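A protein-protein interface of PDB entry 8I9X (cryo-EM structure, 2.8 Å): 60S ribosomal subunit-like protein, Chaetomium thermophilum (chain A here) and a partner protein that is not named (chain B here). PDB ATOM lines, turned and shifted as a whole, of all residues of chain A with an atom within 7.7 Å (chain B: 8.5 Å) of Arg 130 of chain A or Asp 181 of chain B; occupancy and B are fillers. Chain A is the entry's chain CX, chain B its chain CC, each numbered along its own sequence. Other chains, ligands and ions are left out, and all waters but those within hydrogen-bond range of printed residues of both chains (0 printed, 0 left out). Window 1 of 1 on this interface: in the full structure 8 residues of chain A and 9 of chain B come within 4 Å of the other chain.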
ATOM      1  N   THR A 103      32.067 -16.597 -21.022  1.00  0.00           N
ATOM      2  CA  THR A 103      30.638 -16.893 -21.113  1.00  0.00           C
ATOM      3  C   THR A 103      29.962 -16.027 -22.173  1.00  0.00           C
ATOM      4  O   THR A 103      29.121 -16.515 -22.946  1.00  0.00           O
ATOM      5  CB  THR A 103      29.952 -16.734 -19.751  1.00  0.00           C
ATOM      6  OG1 THR A 103      28.545 -16.963 -19.898  1.00  0.00           O
ATOM      7  CG2 THR A 103      30.157 -15.359 -19.191  1.00  0.00           C
ATOM      8  N   ALA A 106      30.921 -17.534 -25.451  1.00  0.00           N
ATOM      9  CA  ALA A 106      30.213 -18.780 -25.712  1.00  0.00           C
ATOM     10  C   ALA A 106      28.803 -18.510 -26.209  1.00  0.00           C
ATOM     11  O   ALA A 106      28.357 -19.121 -27.188  1.00  0.00           O
ATOM     12  CB  ALA A 106      30.184 -19.643 -24.453  1.00  0.00           C
ATOM     13  N   ARG A 122      24.458 -30.141 -30.379  1.00  0.00           N
ATOM     14  CA  ARG A 122      23.668 -29.107 -29.716  1.00  0.00           C
ATOM     15  C   ARG A 122      23.804 -29.200 -28.199  1.00  0.00           C
ATOM     16  O   ARG A 122      23.950 -28.176 -27.510  1.00  0.00           O
ATOM     17  CB  ARG A 122      22.204 -29.222 -30.136  1.00  0.00           C
ATOM     18  CG  ARG A 122      21.979 -29.013 -31.623  1.00  0.00           C
ATOM     19  CD  ARG A 122      20.510 -28.820 -31.949  1.00  0.00           C
ATOM     20  NE  ARG A 122      19.713 -29.986 -31.589  1.00  0.00           N
ATOM     21  CZ  ARG A 122      18.863 -30.592 -32.406  1.00  0.00           C
ATOM     22  NH1 ARG A 122      18.685 -30.177 -33.649  1.00  0.00           N
ATOM     23  NH2 ARG A 122      18.177 -31.642 -31.966  1.00  0.00           N
ATOM     24  N   ALA A 123      23.772 -30.423 -27.667  1.00  0.00           N
ATOM     25  CA  ALA A 123      23.926 -30.616 -26.231  1.00  0.00           C
ATOM     26  C   ALA A 123      25.281 -30.119 -25.747  1.00  0.00           C
ATOM     27  O   ALA A 123      25.373 -29.499 -24.686  1.00  0.00           O
ATOM     28  CB  ALA A 123      23.736 -32.089 -25.877  1.00  0.00           C
ATOM     29  N   ARG A 124      26.347 -30.383 -26.507  1.00  0.00           N
ATOM     30  CA  ARG A 124      27.673 -29.924 -26.106  1.00  0.00           C
ATOM     31  C   ARG A 124      27.788 -28.408 -26.153  1.00  0.00           C
ATOM     32  O   ARG A 124      28.459 -27.814 -25.303  1.00  0.00           O
ATOM     33  CB  ARG A 124      28.757 -30.555 -26.979  1.00  0.00           C
ATOM     34  CG  ARG A 124      28.721 -32.061 -27.012  1.00  0.00           C
ATOM     35  CD  ARG A 124      29.794 -32.666 -26.145  1.00  0.00           C
ATOM     36  NE  ARG A 124      29.417 -34.001 -25.702  1.00  0.00           N
ATOM     37  CZ  ARG A 124      30.272 -34.908 -25.253  1.00  0.00           C
ATOM     38  NH1 ARG A 124      31.568 -34.657 -25.176  1.00  0.00           N
ATOM     39  NH2 ARG A 124      29.815 -36.097 -24.870  1.00  0.00           N
ATOM     40  N   GLN A 125      27.159 -27.768 -27.139  1.00  0.00           N
ATOM     41  CA  GLN A 125      27.153 -26.308 -27.172  1.00  0.00           C
ATOM     42  C   GLN A 125      26.471 -25.742 -25.928  1.00  0.00           C
ATOM     43  O   GLN A 125      27.008 -24.852 -25.243  1.00  0.00           O
ATOM     44  CB  GLN A 125      26.451 -25.836 -28.446  1.00  0.00           C
ATOM     45  CG  GLN A 125      26.635 -24.374 -28.777  1.00  0.00           C
ATOM     46  CD  GLN A 125      26.381 -24.089 -30.243  1.00  0.00           C
ATOM     47  OE1 GLN A 125      25.249 -24.176 -30.716  1.00  0.00           O
ATOM     48  NE2 GLN A 125      27.437 -23.752 -30.971  1.00  0.00           N
ATOM     49  N   LEU A 126      25.297 -26.283 -25.597  1.00  0.00           N
ATOM     50  CA  LEU A 126      24.610 -25.829 -24.395  1.00  0.00           C
ATOM     51  C   LEU A 126      25.431 -26.119 -23.144  1.00  0.00           C
ATOM     52  O   LEU A 126      25.484 -25.285 -22.235  1.00  0.00           O
ATOM     53  CB  LEU A 126      23.229 -26.472 -24.303  1.00  0.00           C
ATOM     54  CG  LEU A 126      22.203 -25.908 -25.289  1.00  0.00           C
ATOM     55  CD1 LEU A 126      21.012 -26.841 -25.430  1.00  0.00           C
ATOM     56  CD2 LEU A 126      21.761 -24.512 -24.888  1.00  0.00           C
ATOM     57  N   GLU A 127      26.090 -27.277 -23.088  1.00  0.00           N
ATOM     58  CA  GLU A 127      26.912 -27.633 -21.938  1.00  0.00           C
ATOM     59  C   GLU A 127      28.112 -26.714 -21.770  1.00  0.00           C
ATOM     60  O   GLU A 127      28.477 -26.399 -20.636  1.00  0.00           O
ATOM     61  CB  GLU A 127      27.387 -29.083 -22.048  1.00  0.00           C
ATOM     62  CG  GLU A 127      26.302 -30.118 -21.805  1.00  0.00           C
ATOM     63  CD  GLU A 127      25.840 -30.152 -20.362  1.00  0.00           C
ATOM     64  OE1 GLU A 127      26.665 -29.877 -19.466  1.00  0.00           O
ATOM     65  OE2 GLU A 127      24.652 -30.455 -20.124  1.00  0.00           O
ATOM     66  N   GLU A 128      28.757 -26.296 -22.861  1.00  0.00           N
ATOM     67  CA  GLU A 128      29.874 -25.374 -22.691  1.00  0.00           C
ATOM     68  C   GLU A 128      29.394 -24.010 -22.219  1.00  0.00           C
ATOM     69  O   GLU A 128      30.060 -23.381 -21.386  1.00  0.00           O
ATOM     70  CB  GLU A 128      30.697 -25.249 -23.978  1.00  0.00           C
ATOM     71  CG  GLU A 128      29.997 -24.610 -25.155  1.00  0.00           C
ATOM     72  CD  GLU A 128      30.861 -24.583 -26.398  1.00  0.00           C
ATOM     73  OE1 GLU A 128      32.002 -25.088 -26.342  1.00  0.00           O
ATOM     74  OE2 GLU A 128      30.400 -24.059 -27.434  1.00  0.00           O
ATOM     75  N   ILE A 129      28.229 -23.555 -22.691  1.00  0.00           N
ATOM     76  CA  ILE A 129      27.685 -22.324 -22.114  1.00  0.00           C
ATOM     77  C   ILE A 129      27.393 -22.501 -20.622  1.00  0.00           C
ATOM     78  O   ILE A 129      27.693 -21.612 -19.808  1.00  0.00           O
ATOM     79  CB  ILE A 129      26.431 -21.869 -22.878  1.00  0.00           C
ATOM     80  CG1 ILE A 129      26.750 -21.673 -24.357  1.00  0.00           C
ATOM     81  CG2 ILE A 129      25.898 -20.578 -22.290  1.00  0.00           C
ATOM     82  CD1 ILE A 129      25.648 -20.993 -25.124  1.00  0.00           C
ATOM     83  N   ARG A 130      26.805 -23.638 -20.241  1.00  0.00           N
ATOM     84  CA  ARG A 130      26.489 -23.887 -18.836  1.00  0.00           C
ATOM     85  C   ARG A 130      27.744 -23.925 -17.977  1.00  0.00           C
ATOM     86  O   ARG A 130      27.762 -23.379 -16.869  1.00  0.00           O
ATOM     87  CB  ARG A 130      25.714 -25.196 -18.692  1.00  0.00           C
ATOM     88  CG  ARG A 130      24.376 -25.226 -19.404  1.00  0.00           C
ATOM     89  CD  ARG A 130      23.674 -26.553 -19.194  1.00  0.00           C
ATOM     90  NE  ARG A 130      22.507 -26.692 -20.055  1.00  0.00           N
ATOM     91  CZ  ARG A 130      22.175 -27.807 -20.690  1.00  0.00           C
ATOM     92  NH1 ARG A 130      22.902 -28.905 -20.584  1.00  0.00           N
ATOM     93  NH2 ARG A 130      21.086 -27.818 -21.452  1.00  0.00           N
ATOM     94  N   GLU A 131      28.801 -24.573 -18.465  1.00  0.00           N
ATOM     95  CA  GLU A 131      30.056 -24.626 -17.727  1.00  0.00           C
ATOM     96  C   GLU A 131      30.688 -23.250 -17.593  1.00  0.00           C
ATOM     97  O   GLU A 131      31.258 -22.936 -16.541  1.00  0.00           O
ATOM     98  CB  GLU A 131      31.028 -25.590 -18.408  1.00  0.00           C
ATOM     99  CG  GLU A 131      31.066 -26.973 -17.783  1.00  0.00           C
ATOM    100  CD  GLU A 131      31.662 -26.969 -16.389  1.00  0.00           C
ATOM    101  OE1 GLU A 131      32.447 -26.048 -16.078  1.00  0.00           O
ATOM    102  OE2 GLU A 131      31.345 -27.887 -15.603  1.00  0.00           O
ATOM    103  N   ALA A 132      30.602 -22.423 -18.639  1.00  0.00           N
ATOM    104  CA  ALA A 132      31.076 -21.050 -18.516  1.00  0.00           C
ATOM    105  C   ALA A 132      30.333 -20.301 -17.419  1.00  0.00           C
ATOM    106  O   ALA A 132      30.963 -19.629 -16.591  1.00  0.00           O
ATOM    107  CB  ALA A 132      30.933 -20.325 -19.852  1.00  0.00           C
ATOM    108  N   ARG A 133      29.000 -20.413 -17.385  1.00  0.00           N
ATOM    109  CA  ARG A 133      28.253 -19.750 -16.318  1.00  0.00           C
ATOM    110  C   ARG A 133      28.616 -20.298 -14.943  1.00  0.00           C
ATOM    111  O   ARG A 133      28.708 -19.533 -13.976  1.00  0.00           O
ATOM    112  CB  ARG A 133      26.747 -19.875 -16.539  1.00  0.00           C
ATOM    113  CG  ARG A 133      26.201 -19.077 -17.701  1.00  0.00           C
ATOM    114  CD  ARG A 133      24.686 -19.089 -17.665  1.00  0.00           C
ATOM    115  NE  ARG A 133      24.091 -18.690 -18.934  1.00  0.00           N
ATOM    116  CZ  ARG A 133      23.758 -17.447 -19.249  1.00  0.00           C
ATOM    117  NH1 ARG A 133      23.953 -16.445 -18.409  1.00  0.00           N
ATOM    118  NH2 ARG A 133      23.212 -17.203 -20.437  1.00  0.00           N
ATOM    119  N   ARG A 134      28.813 -21.613 -14.838  1.00  0.00           N
ATOM    120  CA  ARG A 134      29.176 -22.215 -13.560  1.00  0.00           C
ATOM    121  C   ARG A 134      30.517 -21.694 -13.059  1.00  0.00           C
ATOM    122  O   ARG A 134      30.654 -21.351 -11.878  1.00  0.00           O
ATOM    123  CB  ARG A 134      29.209 -23.735 -13.697  1.00  0.00           C
ATOM    124  CG  ARG A 134      29.102 -24.487 -12.386  1.00  0.00           C
ATOM    125  CD  ARG A 134      29.266 -25.981 -12.613  1.00  0.00           C
ATOM    126  NE  ARG A 134      30.643 -26.368 -12.902  1.00  0.00           N
ATOM    127  CZ  ARG A 134      31.676 -26.189 -12.088  1.00  0.00           C
ATOM    128  NH1 ARG A 134      31.527 -25.674 -10.878  1.00  0.00           N
ATOM    129  NH2 ARG A 134      32.888 -26.553 -12.492  1.00  0.00           N
ATOM    130  N   ILE A 135      31.513 -21.617 -13.941  1.00  0.00           N
ATOM    131  CA  ILE A 135      32.820 -21.112 -13.534  1.00  0.00           C
ATOM    132  C   ILE A 135      32.734 -19.636 -13.163  1.00  0.00           C
ATOM    133  O   ILE A 135      33.368 -19.190 -12.197  1.00  0.00           O
ATOM    134  CB  ILE A 135      33.864 -21.364 -14.637  1.00  0.00           C
ATOM    135  CG1 ILE A 135      34.011 -22.861 -14.902  1.00  0.00           C
ATOM    136  CG2 ILE A 135      35.208 -20.783 -14.242  1.00  0.00           C
ATOM    137  CD1 ILE A 135      34.642 -23.182 -16.237  1.00  0.00           C
ATOM    138  N   GLU A 136      31.953 -18.854 -13.917  1.00  0.00           N
ATOM    139  CA  GLU A 136      31.780 -17.446 -13.569  1.00  0.00           C
ATOM    140  C   GLU A 136      31.177 -17.291 -12.181  1.00  0.00           C
ATOM    141  O   GLU A 136      31.654 -16.484 -11.371  1.00  0.00           O
ATOM    142  CB  GLU A 136      30.886 -16.746 -14.588  1.00  0.00           C
ATOM    143  CG  GLU A 136      30.738 -15.256 -14.319  1.00  0.00           C
ATOM    144  CD  GLU A 136      29.886 -14.559 -15.353  1.00  0.00           C
ATOM    145  OE1 GLU A 136      29.392 -15.246 -16.266  1.00  0.00           O
ATOM    146  OE2 GLU A 136      29.713 -13.326 -15.255  1.00  0.00           O
ATOM    147  N   ALA A 137      30.117 -18.048 -11.893  1.00  0.00           N
ATOM    148  CA  ALA A 137      29.478 -17.979 -10.587  1.00  0.00           C
ATOM    149  C   ALA A 137      30.432 -18.399  -9.478  1.00  0.00           C
ATOM    150  O   ALA A 137      30.469 -17.765  -8.416  1.00  0.00           O
ATOM    151  CB  ALA A 137      28.222 -18.849 -10.569  1.00  0.00           C
ATOM    152  N   PRO B 176       7.649 -23.553 -21.063  1.00  0.00           N
ATOM    153  CA  PRO B 176       8.591 -24.429 -21.764  1.00  0.00           C
ATOM    154  C   PRO B 176       9.951 -24.443 -21.089  1.00  0.00           C
ATOM    155  O   PRO B 176      10.352 -23.487 -20.422  1.00  0.00           O
ATOM    156  CB  PRO B 176       8.681 -23.810 -23.163  1.00  0.00           C
ATOM    157  CG  PRO B 176       7.464 -22.962 -23.293  1.00  0.00           C
ATOM    158  CD  PRO B 176       7.182 -22.452 -21.920  1.00  0.00           C
ATOM    159  N   LEU B 177      10.663 -25.552 -21.270  1.00  0.00           N
ATOM    160  CA  LEU B 177      12.047 -25.663 -20.841  1.00  0.00           C
ATOM    161  C   LEU B 177      13.024 -25.154 -21.892  1.00  0.00           C
ATOM    162  O   LEU B 177      14.200 -25.532 -21.867  1.00  0.00           O
ATOM    163  CB  LEU B 177      12.379 -27.107 -20.460  1.00  0.00           C
ATOM    164  CG  LEU B 177      11.970 -27.569 -19.059  1.00  0.00           C
ATOM    165  CD1 LEU B 177      10.463 -27.753 -18.938  1.00  0.00           C
ATOM    166  CD2 LEU B 177      12.700 -28.847 -18.685  1.00  0.00           C
ATOM    167  N   SER B 178      12.557 -24.330 -22.833  1.00  0.00           N
ATOM    168  CA  SER B 178      13.482 -23.590 -23.682  1.00  0.00           C
ATOM    169  C   SER B 178      14.297 -22.606 -22.859  1.00  0.00           C
ATOM    170  O   SER B 178      15.457 -22.332 -23.184  1.00  0.00           O
ATOM    171  CB  SER B 178      12.722 -22.866 -24.791  1.00  0.00           C
ATOM    172  OG  SER B 178      11.818 -23.739 -25.443  1.00  0.00           O
ATOM    173  N   PHE B 179      13.703 -22.056 -21.806  1.00  0.00           N
ATOM    174  CA  PHE B 179      14.480 -21.409 -20.767  1.00  0.00           C
ATOM    175  C   PHE B 179      15.339 -22.449 -20.056  1.00  0.00           C
ATOM    176  O   PHE B 179      15.093 -23.655 -20.140  1.00  0.00           O
ATOM    177  CB  PHE B 179      13.563 -20.708 -19.764  1.00  0.00           C
ATOM    178  CG  PHE B 179      12.495 -19.865 -20.399  1.00  0.00           C
ATOM    179  CD1 PHE B 179      12.742 -18.543 -20.724  1.00  0.00           C
ATOM    180  CD2 PHE B 179      11.243 -20.390 -20.665  1.00  0.00           C
ATOM    181  CE1 PHE B 179      11.763 -17.763 -21.304  1.00  0.00           C
ATOM    182  CE2 PHE B 179      10.261 -19.613 -21.247  1.00  0.00           C
ATOM    183  CZ  PHE B 179      10.523 -18.299 -21.567  1.00  0.00           C
ATOM    184  N   TYR B 180      16.364 -21.970 -19.361  1.00  0.00           N
ATOM    185  CA  TYR B 180      17.336 -22.800 -18.653  1.00  0.00           C
ATOM    186  C   TYR B 180      18.201 -23.637 -19.587  1.00  0.00           C
ATOM    187  O   TYR B 180      19.017 -24.433 -19.109  1.00  0.00           O
ATOM    188  CB  TYR B 180      16.672 -23.730 -17.626  1.00  0.00           C
ATOM    189  CG  TYR B 180      15.784 -23.058 -16.609  1.00  0.00           C
ATOM    190  CD1 TYR B 180      16.307 -22.568 -15.424  1.00  0.00           C
ATOM    191  CD2 TYR B 180      14.417 -22.956 -16.812  1.00  0.00           C
ATOM    192  CE1 TYR B 180      15.500 -21.968 -14.483  1.00  0.00           C
ATOM    193  CE2 TYR B 180      13.602 -22.359 -15.875  1.00  0.00           C
ATOM    194  CZ  TYR B 180      14.149 -21.869 -14.711  1.00  0.00           C
ATOM    195  OH  TYR B 180      13.344 -21.270 -13.773  1.00  0.00           O
ATOM    196  N   ASP B 181      18.045 -23.494 -20.905  1.00  0.00           N
ATOM    197  CA  ASP B 181      18.877 -24.267 -21.822  1.00  0.00           C
ATOM    198  C   ASP B 181      20.350 -23.926 -21.660  1.00  0.00           C
ATOM    199  O   ASP B 181      21.206 -24.815 -21.728  1.00  0.00           O
ATOM    200  CB  ASP B 181      18.443 -24.043 -23.270  1.00  0.00           C
ATOM    201  CG  ASP B 181      17.190 -24.812 -23.631  1.00  0.00           C
ATOM    202  OD1 ASP B 181      16.897 -25.822 -22.958  1.00  0.00           O
ATOM    203  OD2 ASP B 181      16.512 -24.423 -24.605  1.00  0.00           O
ATOM    204  N   SER B 182      20.663 -22.654 -21.438  1.00  0.00           N
ATOM    205  CA  SER B 182      22.032 -22.214 -21.233  1.00  0.00           C
ATOM    206  C   SER B 182      22.354 -21.969 -19.765  1.00  0.00           C
ATOM    207  O   SER B 182      23.205 -21.129 -19.461  1.00  0.00           O
ATOM    208  CB  SER B 182      22.304 -20.950 -22.050  1.00  0.00           C
ATOM    209  OG  SER B 182      21.355 -19.943 -21.759  1.00  0.00           O
ATOM    210  N   TYR B 183      21.702 -22.684 -18.853  1.00  0.00           N
ATOM    211  CA  TYR B 183      21.915 -22.460 -17.437  1.00  0.00           C
ATOM    212  C   TYR B 183      22.287 -23.761 -16.737  1.00  0.00           C
ATOM    213  O   TYR B 183      21.817 -24.836 -17.119  1.00  0.00           O
ATOM    214  CB  TYR B 183      20.662 -21.867 -16.780  1.00  0.00           C
ATOM    215  CG  TYR B 183      20.423 -20.420 -17.132  1.00  0.00           C
ATOM    216  CD1 TYR B 183      20.978 -19.401 -16.371  1.00  0.00           C
ATOM    217  CD2 TYR B 183      19.652 -20.072 -18.230  1.00  0.00           C
ATOM    218  CE1 TYR B 183      20.764 -18.079 -16.691  1.00  0.00           C
ATOM    219  CE2 TYR B 183      19.435 -18.752 -18.558  1.00  0.00           C
ATOM    220  CZ  TYR B 183      19.992 -17.760 -17.785  1.00  0.00           C
ATOM    221  OH  TYR B 183      19.776 -16.442 -18.110  1.00  0.00           O
ATOM    222  N   PRO B 184      23.136 -23.693 -15.707  1.00  0.00           N
ATOM    223  CA  PRO B 184      23.512 -24.912 -14.979  1.00  0.00           C
ATOM    224  C   PRO B 184      22.387 -25.496 -14.151  1.00  0.00           C
ATOM    225  O   PRO B 184      22.517 -26.630 -13.676  1.00  0.00           O
ATOM    226  CB  PRO B 184      24.664 -24.445 -14.077  1.00  0.00           C
ATOM    227  CG  PRO B 184      25.032 -23.075 -14.557  1.00  0.00           C
ATOM    228  CD  PRO B 184      23.800 -22.503 -15.160  1.00  0.00           C
ATOM    229  N   HIS B 185      21.297 -24.763 -13.956  1.00  0.00           N
ATOM    230  CA  HIS B 185      20.222 -25.155 -13.063  1.00  0.00           C
ATOM    231  C   HIS B 185      18.907 -25.236 -13.826  1.00  0.00           C
ATOM    232  O   HIS B 185      18.755 -24.685 -14.920  1.00  0.00           O
ATOM    233  CB  HIS B 185      20.100 -24.170 -11.896  1.00  0.00           C
ATOM    234  CG  HIS B 185      19.647 -22.805 -12.305  1.00  0.00           C
ATOM    235  ND1 HIS B 185      18.366 -22.349 -12.086  1.00  0.00           N
ATOM    236  CD2 HIS B 185      20.305 -21.797 -12.924  1.00  0.00           C
ATOM    237  CE1 HIS B 185      18.254 -21.118 -12.552  1.00  0.00           C
ATOM    238  NE2 HIS B 185      19.415 -20.759 -13.065  1.00  0.00           N
ATOM    239  N   ILE B 186      17.952 -25.948 -13.235  1.00  0.00           N
ATOM    240  CA  ILE B 186      16.609 -26.098 -13.784  1.00  0.00           C
ATOM    241  C   ILE B 186      15.610 -25.799 -12.667  1.00  0.00           C
ATOM    242  O   ILE B 186      15.278 -26.670 -11.856  1.00  0.00           O
ATOM    243  CB  ILE B 186      16.384 -27.486 -14.411  1.00  0.00           C
ATOM    244  CG1 ILE B 186      15.020 -27.563 -15.106  1.00  0.00           C
ATOM    245  CG2 ILE B 186      16.664 -28.642 -13.432  1.00  0.00           C
ATOM    246  CD1 ILE B 186      14.897 -26.662 -16.314  1.00  0.00           C
ATOM    247  N   MET B 196      20.003 -27.856  -9.372  1.00  0.00           N
ATOM    248  CA  MET B 196      21.105 -28.007 -10.305  1.00  0.00           C
ATOM    249  C   MET B 196      20.896 -29.230 -11.193  1.00  0.00           C
ATOM    250  O   MET B 196      20.364 -30.258 -10.765  1.00  0.00           O
ATOM    251  CB  MET B 196      22.428 -28.122  -9.550  1.00  0.00           C
ATOM    252  CG  MET B 196      22.654 -27.025  -8.517  1.00  0.00           C
ATOM    253  SD  MET B 196      22.871 -25.353  -9.163  1.00  0.00           S
ATOM    254  CE  MET B 196      23.668 -25.656 -10.736  1.00  0.00           C
ATOM    255  N   ARG B 197      21.314 -29.101 -12.450  1.00  0.00           N
ATOM    256  CA  ARG B 197      21.225 -30.215 -13.380  1.00  0.00           C
ATOM    257  C   ARG B 197      22.114 -31.362 -12.903  1.00  0.00           C
ATOM    258  O   ARG B 197      23.213 -31.125 -12.393  1.00  0.00           O
ATOM    259  CB  ARG B 197      21.634 -29.778 -14.784  1.00  0.00           C
ATOM    260  CG  ARG B 197      20.753 -28.694 -15.368  1.00  0.00           C
ATOM    261  CD  ARG B 197      20.747 -28.741 -16.879  1.00  0.00           C
ATOM    262  NE  ARG B 197      19.961 -27.656 -17.452  1.00  0.00           N
ATOM    263  CZ  ARG B 197      19.252 -27.757 -18.566  1.00  0.00           C
ATOM    264  NH1 ARG B 197      19.197 -28.887 -19.250  1.00  0.00           N
ATOM    265  NH2 ARG B 197      18.580 -26.698 -19.004  1.00  0.00           N
ATOM    266  N   PRO B 198      21.666 -32.610 -13.046  1.00  0.00           N
ATOM    267  CA  PRO B 198      22.366 -33.728 -12.400  1.00  0.00           C
ATOM    268  C   PRO B 198      23.781 -33.956 -12.905  1.00  0.00           C
ATOM    269  O   PRO B 198      24.738 -33.904 -12.126  1.00  0.00           O
ATOM    270  CB  PRO B 198      21.472 -34.931 -12.725  1.00  0.00           C
ATOM    271  CG  PRO B 198      20.733 -34.532 -13.952  1.00  0.00           C
ATOM    272  CD  PRO B 198      20.516 -33.059 -13.847  1.00  0.00           C
ATOM    273  N   ALA B 199      23.922 -34.193 -14.203  1.00  0.00           N
ATOM    274  CA  ALA B 199      25.199 -34.565 -14.803  1.00  0.00           C
ATOM    275  C   ALA B 199      25.016 -34.564 -16.313  1.00  0.00           C
ATOM    276  O   ALA B 199      23.964 -34.178 -16.832  1.00  0.00           O
ATOM    277  CB  ALA B 199      25.685 -35.926 -14.304  1.00  0.00           C
ATOM    278  N   THR B 200      26.053 -35.002 -17.018  1.00  0.00           N
ATOM    279  CA  THR B 200      26.018 -35.130 -18.466  1.00  0.00           C
ATOM    280  C   THR B 200      26.084 -36.601 -18.857  1.00  0.00           C
ATOM    281  O   THR B 200      26.864 -37.374 -18.291  1.00  0.00           O
ATOM    282  CB  THR B 200      27.160 -34.340 -19.123  1.00  0.00           C
ATOM    283  OG1 THR B 200      27.030 -34.399 -20.550  1.00  0.00           O
ATOM    284  CG2 THR B 200      28.528 -34.875 -18.704  1.00  0.00           C
ATOM    285  N   GLY B 201      25.227 -36.992 -19.800  1.00  0.00           N
ATOM    286  CA  GLY B 201      25.256 -38.346 -20.300  1.00  0.00           C
ATOM    287  C   GLY B 201      26.381 -38.571 -21.290  1.00  0.00           C
ATOM    288  O   GLY B 201      26.803 -37.670 -22.014  1.00  0.00           O
ATOM    289  N   THR B 221      11.360 -34.426 -21.902  1.00  0.00           N
ATOM    290  CA  THR B 221      12.383 -34.069 -20.930  1.00  0.00           C
ATOM    291  C   THR B 221      11.731 -33.794 -19.582  1.00  0.00           C
ATOM    292  O   THR B 221      10.750 -33.049 -19.502  1.00  0.00           O
ATOM    293  CB  THR B 221      13.176 -32.848 -21.396  1.00  0.00           C
ATOM    294  OG1 THR B 221      13.843 -33.152 -22.627  1.00  0.00           O
ATOM    295  CG2 THR B 221      14.210 -32.451 -20.355  1.00  0.00           C
ATOM    296  N   GLY B 226      17.085 -32.580 -15.672  1.00  0.00           N
ATOM    297  CA  GLY B 226      17.277 -32.353 -17.095  1.00  0.00           C
ATOM    298  C   GLY B 226      17.317 -33.608 -17.941  1.00  0.00           C
ATOM    299  O   GLY B 226      17.151 -33.511 -19.163  1.00  0.00           O
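The guanidinium group (NH1) of Arg 197 of chain B lies close to the guanidinium group (NH2) of Arg 130 of chain A, 3.1 Å away. O of Asp 181 of chain B lies within hydrogen-bond range of NE of Arg 130 of chain A (2.8 Å). The backbone carbonyl oxygen (O) of Ser 182 of chain B is in hydrogen-bond range of the guanidinium group (NE) of Arg 133 of chain A, 2.6 Å away.
The backbone NH of Arg 197 of chain B is in hydrogen-bond range of the backbone carbonyl oxygen of Pro 184 of chain B (3.0 Å). The backbone carbonyl oxygen (O) of Ser 178 of chain B lies close to the side-chain carboxylate (OD2) of Asp 181 of chain B (2.7 Å). The backbone carbonyl oxygen of Tyr 183 of chain B is in hydrogen-bond range of the guanidinium group of Arg 197 of chain B, 3.4 Å away.
Among the printed residues, pairs that only touch across the chains: Leu 126 of chain A with Asp 181 of chain B, Arg 130 of chain A with Tyr 183 of chain B, Arg 130 of chain A with Pro 184 of chain B, Ile 129 of chain A with Ser 182 of chain B, Arg 130 of chain A with Ser 182 of chain B and Arg 133 of chain A with Tyr 183 of chain B.
Printed residues of chain B within 4 Å of Arg 133 of chain A: Ser 182 (2.6 Å) and Tyr 183 (3.9 Å). Asp 181 of chain B touches just these residues of chain A: Leu 126 (3.2 Å) and Arg 130 (2.8 Å). Of the printed residues of chain A, Ser 182 of chain B touches Ile 129 (3.6 Å), Arg 130 (3.9 Å) and Arg 133 (2.6 Å). The nearest residue of chain B that does not touch Arg 130 of chain A is Tyr 180 of chain B (4.3 Å).
Printed residues of chain A that touch a printed residue of chain B: Leu 126, Ile 129, Arg 130 and Arg 133. Hydrophobic or aromatic side chains of chain A within 4 Å of the printed part of chain B: Leu 126 and Ile 129. Of the 19 printed residues of chain B, 5 touch a printed residue of chain A. Among the printed residues, no Asp or Glu carboxylate lies within 4 Å of a Lys or Arg side-chain nitrogen of the other chain.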
